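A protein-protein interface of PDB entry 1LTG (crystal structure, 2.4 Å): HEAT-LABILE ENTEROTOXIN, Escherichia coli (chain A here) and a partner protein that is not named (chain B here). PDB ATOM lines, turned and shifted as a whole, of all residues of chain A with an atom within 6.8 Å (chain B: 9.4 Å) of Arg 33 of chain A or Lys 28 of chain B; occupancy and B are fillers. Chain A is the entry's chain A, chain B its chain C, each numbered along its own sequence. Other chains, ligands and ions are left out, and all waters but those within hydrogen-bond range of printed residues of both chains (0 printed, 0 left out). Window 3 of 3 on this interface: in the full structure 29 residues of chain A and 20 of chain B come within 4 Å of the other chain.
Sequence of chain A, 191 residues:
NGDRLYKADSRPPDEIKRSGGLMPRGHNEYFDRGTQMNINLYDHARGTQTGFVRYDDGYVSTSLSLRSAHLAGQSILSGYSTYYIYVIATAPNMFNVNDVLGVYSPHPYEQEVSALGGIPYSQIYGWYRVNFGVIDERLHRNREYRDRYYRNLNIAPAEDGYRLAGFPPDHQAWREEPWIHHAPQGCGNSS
The guanidinium group (NH1) of Arg 33 of chain A sits close to the side-chain amide nitrogen (NE2) of Gln 24 of chain B (2.6 Å). The backbone carbonyl oxygen (O) of Tyr 30 of chain A lies close to the side-chain amide oxygen (OE1) of Gln 24 of chain B.
A ring nitrogen (NE2) of His 27 of chain A is in hydrogen-bond range of the backbone carbonyl oxygen of Tyr 30 of chain A, 2.6 Å away. NE of Arg 21 of chain B lies close to NE2 of Gln 24 of chain B, at 3.2 Å. A ring nitrogen (ND1) of His 27 of chain A sits close to the backbone carbonyl oxygen of Asp 32 of chain A (2.9 Å).
Among the printed residues, merely in contact across the chains: His 27 of chain A with Gln 24 of chain B (3.95 Å), Tyr 30 of chain A with Tyr 23 of chain B (3.4 Å), Phe 31 of chain A with Gln 24 of chain B (3.6 Å), Phe 31 of chain A with Val 27 of chain B (3.9 Å), Phe 31 of chain A with Lys 28 of chain B (3.99 Å), Arg 33 of chain A with Arg 21 of chain B (3.4 Å) and Arg 33 of chain A with Lys 28 of chain B (3.7 Å).
Arg 33 of chain A touches just these residues of chain B: Arg 21, Gln 24 and Lys 28. Printed residues of chain A within 4 Å of Lys 28 of chain B: Phe 31 (3.99 Å) and Arg 33 (3.7 Å). No residue of chain B comes within 4 Å of Asp 32 of chain A. No residue of chain B comes within 4 Å of Gly 34 of chain A. Of the printed residues of chain A, Arg 21 of chain B touches Arg 33 (3.4 Å). Of the printed residues of chain A, Val 27 of chain B touches Phe 31 (3.9 Å). Printed residues of chain A within 4 Å of Gln 24 of chain B: His 27 (3.95 Å), Tyr 30 (2.9 Å), Phe 31 (3.6 Å) and Arg 33 (2.6 Å). Asn 28 of chain A touches none of the printed residues of chain B. The nearest printed residue of chain A that does not touch Lys 28 of chain B is Tyr 30 of chain A (7.0 Å).
Hydrophobic or aromatic side chains of chain B that line the printed part of chain A: Tyr 23 and Val 27. Of the 10 printed residues of chain A, 4 touch a printed residue of chain B. Printed residues of chain A that touch a printed residue of chain B: His 27, Tyr 30, Phe 31 and Arg 33. Hydrophobic or aromatic side chains of chain A that line the printed part of chain B: His 27, Tyr 30 and Phe 31. Among the printed residues, 9 pairs touch across the chains. Among the printed residues, no Asp or Glu carboxylate lies within 4 Å of a Lys or Arg side-chain nitrogen of the other chain.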
ATOM      1  N   HIS A  27      28.563   1.847  13.586  1.00  0.00           N
ATOM      2  CA  HIS A  27      27.414   1.207  12.972  1.00  0.00           C
ATOM      3  C   HIS A  27      26.365   1.564  14.013  1.00  0.00           C
ATOM      4  O   HIS A  27      26.625   1.443  15.217  1.00  0.00           O
ATOM      5  CB  HIS A  27      27.583  -0.301  12.912  1.00  0.00           C
ATOM      6  CG  HIS A  27      27.441  -0.895  11.517  1.00  0.00           C
ATOM      7  ND1 HIS A  27      27.618  -0.323  10.326  1.00  0.00           N
ATOM      8  CD2 HIS A  27      27.107  -2.217  11.299  1.00  0.00           C
ATOM      9  CE1 HIS A  27      27.402  -1.258   9.413  1.00  0.00           C
ATOM     10  NE2 HIS A  27      27.094  -2.389  10.003  1.00  0.00           N
ATOM     11  N   ASN A  28      25.239   2.129  13.571  1.00  0.00           N
ATOM     12  CA  ASN A  28      24.190   2.552  14.502  1.00  0.00           C
ATOM     13  C   ASN A  28      23.287   1.358  14.787  1.00  0.00           C
ATOM     14  O   ASN A  28      22.704   1.203  15.861  1.00  0.00           O
ATOM     15  CB  ASN A  28      23.301   3.667  13.932  1.00  0.00           C
ATOM     16  CG  ASN A  28      23.894   4.665  12.940  1.00  0.00           C
ATOM     17  OD1 ASN A  28      23.216   4.944  11.956  1.00  0.00           O
ATOM     18  ND2 ASN A  28      25.099   5.230  13.060  1.00  0.00           N
ATOM     19  N   GLU A  29      23.144   0.563  13.726  1.00  0.00           N
ATOM     20  CA  GLU A  29      22.476  -0.714  13.707  1.00  0.00           C
ATOM     21  C   GLU A  29      23.269  -1.497  12.653  1.00  0.00           C
ATOM     22  O   GLU A  29      24.210  -0.956  12.046  1.00  0.00           O
ATOM     23  CB  GLU A  29      20.995  -0.527  13.316  1.00  0.00           C
ATOM     24  CG  GLU A  29      20.550  -0.387  11.851  1.00  0.00           C
ATOM     25  CD  GLU A  29      20.515   0.997  11.201  1.00  0.00           C
ATOM     26  OE1 GLU A  29      20.946   1.988  11.801  1.00  0.00           O
ATOM     27  OE2 GLU A  29      20.042   1.075  10.061  1.00  0.00           O
ATOM     28  N   TYR A  30      22.962  -2.752  12.359  1.00  0.00           N
ATOM     29  CA  TYR A  30      23.740  -3.562  11.425  1.00  0.00           C
ATOM     30  C   TYR A  30      23.715  -3.194   9.945  1.00  0.00           C
ATOM     31  O   TYR A  30      24.750  -3.338   9.303  1.00  0.00           O
ATOM     32  CB  TYR A  30      23.302  -5.004  11.628  1.00  0.00           C
ATOM     33  CG  TYR A  30      24.143  -6.016  10.919  1.00  0.00           C
ATOM     34  CD1 TYR A  30      25.490  -6.166  11.232  1.00  0.00           C
ATOM     35  CD2 TYR A  30      23.568  -6.778   9.904  1.00  0.00           C
ATOM     36  CE1 TYR A  30      26.278  -7.084  10.513  1.00  0.00           C
ATOM     37  CE2 TYR A  30      24.350  -7.692   9.187  1.00  0.00           C
ATOM     38  CZ  TYR A  30      25.704  -7.841   9.489  1.00  0.00           C
ATOM     39  OH  TYR A  30      26.462  -8.720   8.752  1.00  0.00           O
ATOM     40  N   PHE A  31      22.661  -2.687   9.317  1.00  0.00           N
ATOM     41  CA  PHE A  31      22.747  -2.389   7.900  1.00  0.00           C
ATOM     42  C   PHE A  31      23.023  -0.922   7.629  1.00  0.00           C
ATOM     43  O   PHE A  31      22.783  -0.337   6.566  1.00  0.00           O
ATOM     44  CB  PHE A  31      21.458  -2.816   7.244  1.00  0.00           C
ATOM     45  CG  PHE A  31      21.290  -4.330   7.233  1.00  0.00           C
ATOM     46  CD1 PHE A  31      22.233  -5.148   6.604  1.00  0.00           C
ATOM     47  CD2 PHE A  31      20.190  -4.919   7.870  1.00  0.00           C
ATOM     48  CE1 PHE A  31      22.074  -6.538   6.624  1.00  0.00           C
ATOM     49  CE2 PHE A  31      20.036  -6.310   7.884  1.00  0.00           C
ATOM     50  CZ  PHE A  31      20.981  -7.123   7.262  1.00  0.00           C
ATOM     51  N   ASP A  32      23.568  -0.272   8.637  1.00  0.00           N
ATOM     52  CA  ASP A  32      23.838   1.127   8.556  1.00  0.00           C
ATOM     53  C   ASP A  32      25.080   1.309   7.708  1.00  0.00           C
ATOM     54  O   ASP A  32      26.179   1.018   8.180  1.00  0.00           O
ATOM     55  CB  ASP A  32      24.008   1.642   9.993  1.00  0.00           C
ATOM     56  CG  ASP A  32      24.712   2.984  10.141  1.00  0.00           C
ATOM     57  OD1 ASP A  32      24.196   3.994   9.636  1.00  0.00           O
ATOM     58  OD2 ASP A  32      25.785   2.997  10.756  1.00  0.00           O
ATOM     59  N   ARG A  33      24.921   1.693   6.436  1.00  0.00           N
ATOM     60  CA  ARG A  33      26.067   2.112   5.603  1.00  0.00           C
ATOM     61  C   ARG A  33      26.216   3.647   5.687  1.00  0.00           C
ATOM     62  O   ARG A  33      26.985   4.251   4.926  1.00  0.00           O
ATOM     63  CB  ARG A  33      25.925   1.782   4.091  1.00  0.00           C
ATOM     64  CG  ARG A  33      24.751   0.978   3.519  1.00  0.00           C
ATOM     65  CD  ARG A  33      24.997  -0.522   3.595  1.00  0.00           C
ATOM     66  NE  ARG A  33      24.015  -1.306   2.863  1.00  0.00           N
ATOM     67  CZ  ARG A  33      23.741  -2.558   3.234  1.00  0.00           C
ATOM     68  NH1 ARG A  33      24.346  -3.128   4.264  1.00  0.00           N
ATOM     69  NH2 ARG A  33      22.802  -3.258   2.625  1.00  0.00           N
ATOM     70  N   GLY A  34      25.433   4.300   6.582  1.00  0.00           N
ATOM     71  CA  GLY A  34      25.455   5.741   6.802  1.00  0.00           C
ATOM     72  C   GLY A  34      26.798   6.160   7.385  1.00  0.00           C
ATOM     73  O   GLY A  34      27.511   7.021   6.864  1.00  0.00           O
ATOM     74  N   THR A  35      27.167   5.576   8.515  1.00  0.00           N
ATOM     75  CA  THR A  35      28.495   5.827   9.017  1.00  0.00           C
ATOM     76  C   THR A  35      29.300   4.725   8.328  1.00  0.00           C
ATOM     77  O   THR A  35      28.889   3.552   8.311  1.00  0.00           O
ATOM     78  CB  THR A  35      28.548   5.670  10.549  1.00  0.00           C
ATOM     79  OG1 THR A  35      27.410   6.314  11.159  1.00  0.00           O
ATOM     80  CG2 THR A  35      29.883   6.239  11.044  1.00  0.00           C
ATOM     81  N   GLN A  36      30.367   5.050   7.621  1.00  0.00           N
ATOM     82  CA  GLN A  36      31.203   3.963   7.158  1.00  0.00           C
ATOM     83  C   GLN A  36      32.363   3.918   8.143  1.00  0.00           C
ATOM     84  O   GLN A  36      32.978   4.899   8.573  1.00  0.00           O
ATOM     85  CB  GLN A  36      31.644   4.212   5.718  1.00  0.00           C
ATOM     86  CG  GLN A  36      30.678   3.430   4.802  1.00  0.00           C
ATOM     87  CD  GLN A  36      30.839   3.708   3.304  1.00  0.00           C
ATOM     88  OE1 GLN A  36      31.905   3.532   2.687  1.00  0.00           O
ATOM     89  NE2 GLN A  36      29.744   4.167   2.705  1.00  0.00           N
ATOM     90  N   THR B  17      35.174  -3.814   3.089  1.00  0.00           N
ATOM     91  CA  THR B  17      33.792  -3.451   2.867  1.00  0.00           C
ATOM     92  C   THR B  17      33.128  -4.322   1.788  1.00  0.00           C
ATOM     93  O   THR B  17      31.964  -4.688   1.986  1.00  0.00           O
ATOM     94  CB  THR B  17      33.789  -2.003   2.508  1.00  0.00           C
ATOM     95  OG1 THR B  17      34.320  -1.335   3.645  1.00  0.00           O
ATOM     96  CG2 THR B  17      32.421  -1.466   2.221  1.00  0.00           C
ATOM     97  N   LEU B  20      32.144  -7.520   3.608  1.00  0.00           N
ATOM     98  CA  LEU B  20      30.976  -7.279   4.442  1.00  0.00           C
ATOM     99  C   LEU B  20      29.679  -7.142   3.635  1.00  0.00           C
ATOM    100  O   LEU B  20      28.712  -7.830   3.976  1.00  0.00           O
ATOM    101  CB  LEU B  20      31.206  -6.022   5.300  1.00  0.00           C
ATOM    102  CG  LEU B  20      30.067  -5.583   6.223  1.00  0.00           C
ATOM    103  CD1 LEU B  20      29.744  -6.661   7.241  1.00  0.00           C
ATOM    104  CD2 LEU B  20      30.474  -4.305   6.922  1.00  0.00           C
ATOM    105  N   ARG B  21      29.590  -6.334   2.565  1.00  0.00           N
ATOM    106  CA  ARG B  21      28.375  -6.193   1.756  1.00  0.00           C
ATOM    107  C   ARG B  21      27.896  -7.535   1.184  1.00  0.00           C
ATOM    108  O   ARG B  21      26.682  -7.782   1.139  1.00  0.00           O
ATOM    109  CB  ARG B  21      28.584  -5.242   0.576  1.00  0.00           C
ATOM    110  CG  ARG B  21      28.917  -3.773   0.825  1.00  0.00           C
ATOM    111  CD  ARG B  21      27.833  -2.919   1.482  1.00  0.00           C
ATOM    112  NE  ARG B  21      28.133  -2.662   2.888  1.00  0.00           N
ATOM    113  CZ  ARG B  21      28.315  -1.424   3.392  1.00  0.00           C
ATOM    114  NH1 ARG B  21      28.232  -0.314   2.638  1.00  0.00           N
ATOM    115  NH2 ARG B  21      28.590  -1.280   4.695  1.00  0.00           N
ATOM    116  N   GLU B  22      28.809  -8.450   0.837  1.00  0.00           N
ATOM    117  CA  GLU B  22      28.405  -9.769   0.337  1.00  0.00           C
ATOM    118  C   GLU B  22      27.688 -10.533   1.436  1.00  0.00           C
ATOM    119  O   GLU B  22      26.644 -11.155   1.213  1.00  0.00           O
ATOM    120  CB  GLU B  22      29.574 -10.704  -0.102  1.00  0.00           C
ATOM    121  CG  GLU B  22      30.493 -10.320  -1.280  1.00  0.00           C
ATOM    122  CD  GLU B  22      29.839 -10.026  -2.640  1.00  0.00           C
ATOM    123  OE1 GLU B  22      29.625 -10.950  -3.434  1.00  0.00           O
ATOM    124  OE2 GLU B  22      29.563  -8.855  -2.911  1.00  0.00           O
ATOM    125  N   TYR B  23      28.251 -10.440   2.643  1.00  0.00           N
ATOM    126  CA  TYR B  23      27.708 -11.118   3.779  1.00  0.00           C
ATOM    127  C   TYR B  23      26.347 -10.494   4.070  1.00  0.00           C
ATOM    128  O   TYR B  23      25.368 -11.240   4.224  1.00  0.00           O
ATOM    129  CB  TYR B  23      28.660 -10.981   4.948  1.00  0.00           C
ATOM    130  CG  TYR B  23      28.203 -11.959   6.019  1.00  0.00           C
ATOM    131  CD1 TYR B  23      28.270 -13.335   5.804  1.00  0.00           C
ATOM    132  CD2 TYR B  23      27.677 -11.464   7.212  1.00  0.00           C
ATOM    133  CE1 TYR B  23      27.807 -14.215   6.786  1.00  0.00           C
ATOM    134  CE2 TYR B  23      27.218 -12.341   8.192  1.00  0.00           C
ATOM    135  CZ  TYR B  23      27.288 -13.712   7.974  1.00  0.00           C
ATOM    136  OH  TYR B  23      26.884 -14.566   8.983  1.00  0.00           O
ATOM    137  N   GLN B  24      26.184  -9.174   4.034  1.00  0.00           N
ATOM    138  CA  GLN B  24      24.878  -8.574   4.294  1.00  0.00           C
ATOM    139  C   GLN B  24      23.767  -9.004   3.360  1.00  0.00           C
ATOM    140  O   GLN B  24      22.656  -9.280   3.822  1.00  0.00           O
ATOM    141  CB  GLN B  24      25.014  -7.056   4.288  1.00  0.00           C
ATOM    142  CG  GLN B  24      25.565  -6.644   5.671  1.00  0.00           C
ATOM    143  CD  GLN B  24      25.979  -5.201   5.886  1.00  0.00           C
ATOM    144  OE1 GLN B  24      25.974  -4.698   6.998  1.00  0.00           O
ATOM    145  NE2 GLN B  24      26.429  -4.472   4.880  1.00  0.00           N
ATOM    146  N   SER B  25      23.993  -9.113   2.061  1.00  0.00           N
ATOM    147  CA  SER B  25      22.982  -9.658   1.169  1.00  0.00           C
ATOM    148  C   SER B  25      22.649 -11.093   1.588  1.00  0.00           C
ATOM    149  O   SER B  25      21.459 -11.432   1.642  1.00  0.00           O
ATOM    150  CB  SER B  25      23.473  -9.676  -0.248  1.00  0.00           C
ATOM    151  OG  SER B  25      22.420 -10.230  -1.002  1.00  0.00           O
ATOM    152  N   LYS B  26      23.589 -11.952   1.972  1.00  0.00           N
ATOM    153  CA  LYS B  26      23.204 -13.305   2.367  1.00  0.00           C
ATOM    154  C   LYS B  26      22.290 -13.292   3.609  1.00  0.00           C
ATOM    155  O   LYS B  26      21.303 -14.004   3.783  1.00  0.00           O
ATOM    156  CB  LYS B  26      24.496 -14.060   2.602  1.00  0.00           C
ATOM    157  CG  LYS B  26      24.924 -15.156   1.591  1.00  0.00           C
ATOM    158  CD  LYS B  26      25.186 -14.804   0.117  1.00  0.00           C
ATOM    159  CE  LYS B  26      25.606 -16.085  -0.641  1.00  0.00           C
ATOM    160  NZ  LYS B  26      25.583 -15.947  -2.094  1.00  0.00           N
ATOM    161  N   VAL B  27      22.558 -12.358   4.501  1.00  0.00           N
ATOM    162  CA  VAL B  27      21.795 -12.234   5.709  1.00  0.00           C
ATOM    163  C   VAL B  27      20.429 -11.668   5.297  1.00  0.00           C
ATOM    164  O   VAL B  27      19.431 -12.093   5.909  1.00  0.00           O
ATOM    165  CB  VAL B  27      22.593 -11.311   6.692  1.00  0.00           C
ATOM    166  CG1 VAL B  27      21.740 -10.877   7.866  1.00  0.00           C
ATOM    167  CG2 VAL B  27      23.736 -12.087   7.327  1.00  0.00           C
ATOM    168  N   LYS B  28      20.313 -10.751   4.300  1.00  0.00           N
ATOM    169  CA  LYS B  28      19.027 -10.265   3.827  1.00  0.00           C
ATOM    170  C   LYS B  28      18.291 -11.363   3.078  1.00  0.00           C
ATOM    171  O   LYS B  28      17.068 -11.410   3.189  1.00  0.00           O
ATOM    172  CB  LYS B  28      19.147  -9.110   2.877  1.00  0.00           C
ATOM    173  CG  LYS B  28      19.453  -7.856   3.651  1.00  0.00           C
ATOM    174  CD  LYS B  28      19.221  -6.596   2.853  1.00  0.00           C
ATOM    175  CE  LYS B  28      19.343  -5.458   3.871  1.00  0.00           C
ATOM    176  NZ  LYS B  28      19.254  -4.118   3.303  1.00  0.00           N
ATOM    177  N   ARG B  29      18.902 -12.300   2.339  1.00  0.00           N
ATOM    178  CA  ARG B  29      18.161 -13.365   1.640  1.00  0.00           C
ATOM    179  C   ARG B  29      17.483 -14.277   2.628  1.00  0.00           C
ATOM    180  O   ARG B  29      16.332 -14.675   2.435  1.00  0.00           O
ATOM    181  CB  ARG B  29      19.102 -14.194   0.759  1.00  0.00           C
ATOM    182  CG  ARG B  29      19.475 -13.374  -0.460  1.00  0.00           C
ATOM    183  CD  ARG B  29      20.769 -13.829  -1.021  1.00  0.00           C
ATOM    184  NE  ARG B  29      20.589 -15.127  -1.621  1.00  0.00           N
ATOM    185  CZ  ARG B  29      21.532 -15.733  -2.351  1.00  0.00           C
ATOM    186  NH1 ARG B  29      22.726 -15.184  -2.598  1.00  0.00           N
ATOM    187  NH2 ARG B  29      21.288 -16.956  -2.829  1.00  0.00           N
ATOM    188  N   GLN B  30      18.168 -14.523   3.743  1.00  0.00           N
ATOM    189  CA  GLN B  30      17.634 -15.269   4.861  1.00  0.00           C
ATOM    190  C   GLN B  30      16.423 -14.601   5.511  1.00  0.00           C
ATOM    191  O   GLN B  30      15.312 -15.156   5.493  1.00  0.00           O
ATOM    192  CB  GLN B  30      18.724 -15.459   5.901  1.00  0.00           C
ATOM    193  CG  GLN B  30      19.834 -16.401   5.489  1.00  0.00           C
ATOM    194  CD  GLN B  30      19.285 -17.763   5.139  1.00  0.00           C
ATOM    195  OE1 GLN B  30      18.560 -18.359   5.935  1.00  0.00           O
ATOM    196  NE2 GLN B  30      19.562 -18.292   3.975  1.00  0.00           N
ATOM    197  N   ILE B  31      16.544 -13.379   6.035  1.00  0.00           N
ATOM    198  CA  ILE B  31      15.429 -12.798   6.786  1.00  0.00           C
ATOM    199  C   ILE B  31      14.343 -12.104   5.956  1.00  0.00           C
ATOM    200  O   ILE B  31      13.182 -12.030   6.373  1.00  0.00           O
ATOM    201  CB  ILE B  31      16.005 -11.827   7.870  1.00  0.00           C
ATOM    202  CG1 ILE B  31      16.710 -10.598   7.285  1.00  0.00           C
ATOM    203  CG2 ILE B  31      16.925 -12.694   8.736  1.00  0.00           C
ATOM    204  CD1 ILE B  31      17.466  -9.571   8.179  1.00  0.00           C
ATOM    205  N   PHE B  32      14.598 -11.613   4.748  1.00  0.00           N
ATOM    206  CA  PHE B  32      13.549 -11.006   3.968  1.00  0.00           C
ATOM    207  C   PHE B  32      12.798 -12.081   3.236  1.00  0.00           C
ATOM    208  O   PHE B  32      11.647 -11.864   2.860  1.00  0.00           O
ATOM    209  CB  PHE B  32      14.151  -9.979   2.981  1.00  0.00           C
ATOM    210  CG  PHE B  32      14.605  -8.698   3.695  1.00  0.00           C
ATOM    211  CD1 PHE B  32      14.471  -8.540   5.085  1.00  0.00           C
ATOM    212  CD2 PHE B  32      15.190  -7.664   2.954  1.00  0.00           C
ATOM    213  CE1 PHE B  32      14.923  -7.382   5.721  1.00  0.00           C
ATOM    214  CE2 PHE B  32      15.639  -6.498   3.580  1.00  0.00           C
ATOM    215  CZ  PHE B  32      15.509  -6.360   4.968  1.00  0.00           C
ATOM    216  N   SER B  33      13.341 -13.263   3.005  1.00  0.00           N
ATOM    217  CA  SER B  33      12.542 -14.240   2.311  1.00  0.00           C
ATOM    218  C   SER B  33      11.346 -14.686   3.132  1.00  0.00           C
ATOM    219  O   SER B  33      10.347 -15.127   2.558  1.00  0.00           O
ATOM    220  CB  SER B  33      13.410 -15.403   1.954  1.00  0.00           C
ATOM    221  OG  SER B  33      13.988 -14.967   0.739  1.00  0.00           O
ATOM    222  N   ASP B  34      11.392 -14.482   4.454  1.00  0.00           N
ATOM    223  CA  ASP B  34      10.235 -14.779   5.269  1.00  0.00           C
ATOM    224  C   ASP B  34       8.992 -13.972   4.961  1.00  0.00           C
ATOM    225  O   ASP B  34       7.958 -14.299   5.485  1.00  0.00           O
ATOM    226  CB  ASP B  34      10.516 -14.538   6.711  1.00  0.00           C
ATOM    227  CG  ASP B  34      11.591 -15.418   7.275  1.00  0.00           C
ATOM    228  OD1 ASP B  34      11.862 -16.487   6.715  1.00  0.00           O
ATOM    229  OD2 ASP B  34      12.139 -15.008   8.295  1.00  0.00           O
ATOM    230  N   TYR B  35       9.043 -12.860   4.248  1.00  0.00           N
ATOM    231  CA  TYR B  35       7.844 -12.092   3.986  1.00  0.00           C
ATOM    232  C   TYR B  35       7.386 -12.399   2.570  1.00  0.00           C
ATOM    233  O   TYR B  35       6.387 -11.862   2.141  1.00  0.00           O
ATOM    234  CB  TYR B  35       8.153 -10.624   4.101  1.00  0.00           C
ATOM    235  CG  TYR B  35       8.741 -10.285   5.439  1.00  0.00           C
ATOM    236  CD1 TYR B  35       7.909 -10.223   6.551  1.00  0.00           C
ATOM    237  CD2 TYR B  35      10.107 -10.090   5.556  1.00  0.00           C
ATOM    238  CE1 TYR B  35       8.465  -9.969   7.801  1.00  0.00           C
ATOM    239  CE2 TYR B  35      10.668  -9.839   6.792  1.00  0.00           C
ATOM    240  CZ  TYR B  35       9.846  -9.779   7.908  1.00  0.00           C
ATOM    241  OH  TYR B  35      10.397  -9.509   9.146  1.00  0.00           O
ATOM    242  N   GLN B  36       8.055 -13.277   1.808  1.00  0.00           N
ATOM    243  CA  GLN B  36       7.753 -13.351   0.413  1.00  0.00           C
ATOM    244  C   GLN B  36       6.483 -14.087   0.158  1.00  0.00           C
ATOM    245  O   GLN B  36       6.452 -15.285   0.381  1.00  0.00           O
ATOM    246  CB  GLN B  36       8.892 -14.015  -0.295  1.00  0.00           C
ATOM    247  CG  GLN B  36       9.152 -13.234  -1.571  1.00  0.00           C
ATOM    248  CD  GLN B  36       8.335 -13.632  -2.785  1.00  0.00           C
ATOM    249  OE1 GLN B  36       8.622 -14.677  -3.352  1.00  0.00           O
ATOM    250  NE2 GLN B  36       7.376 -12.897  -3.267  1.00  0.00           N
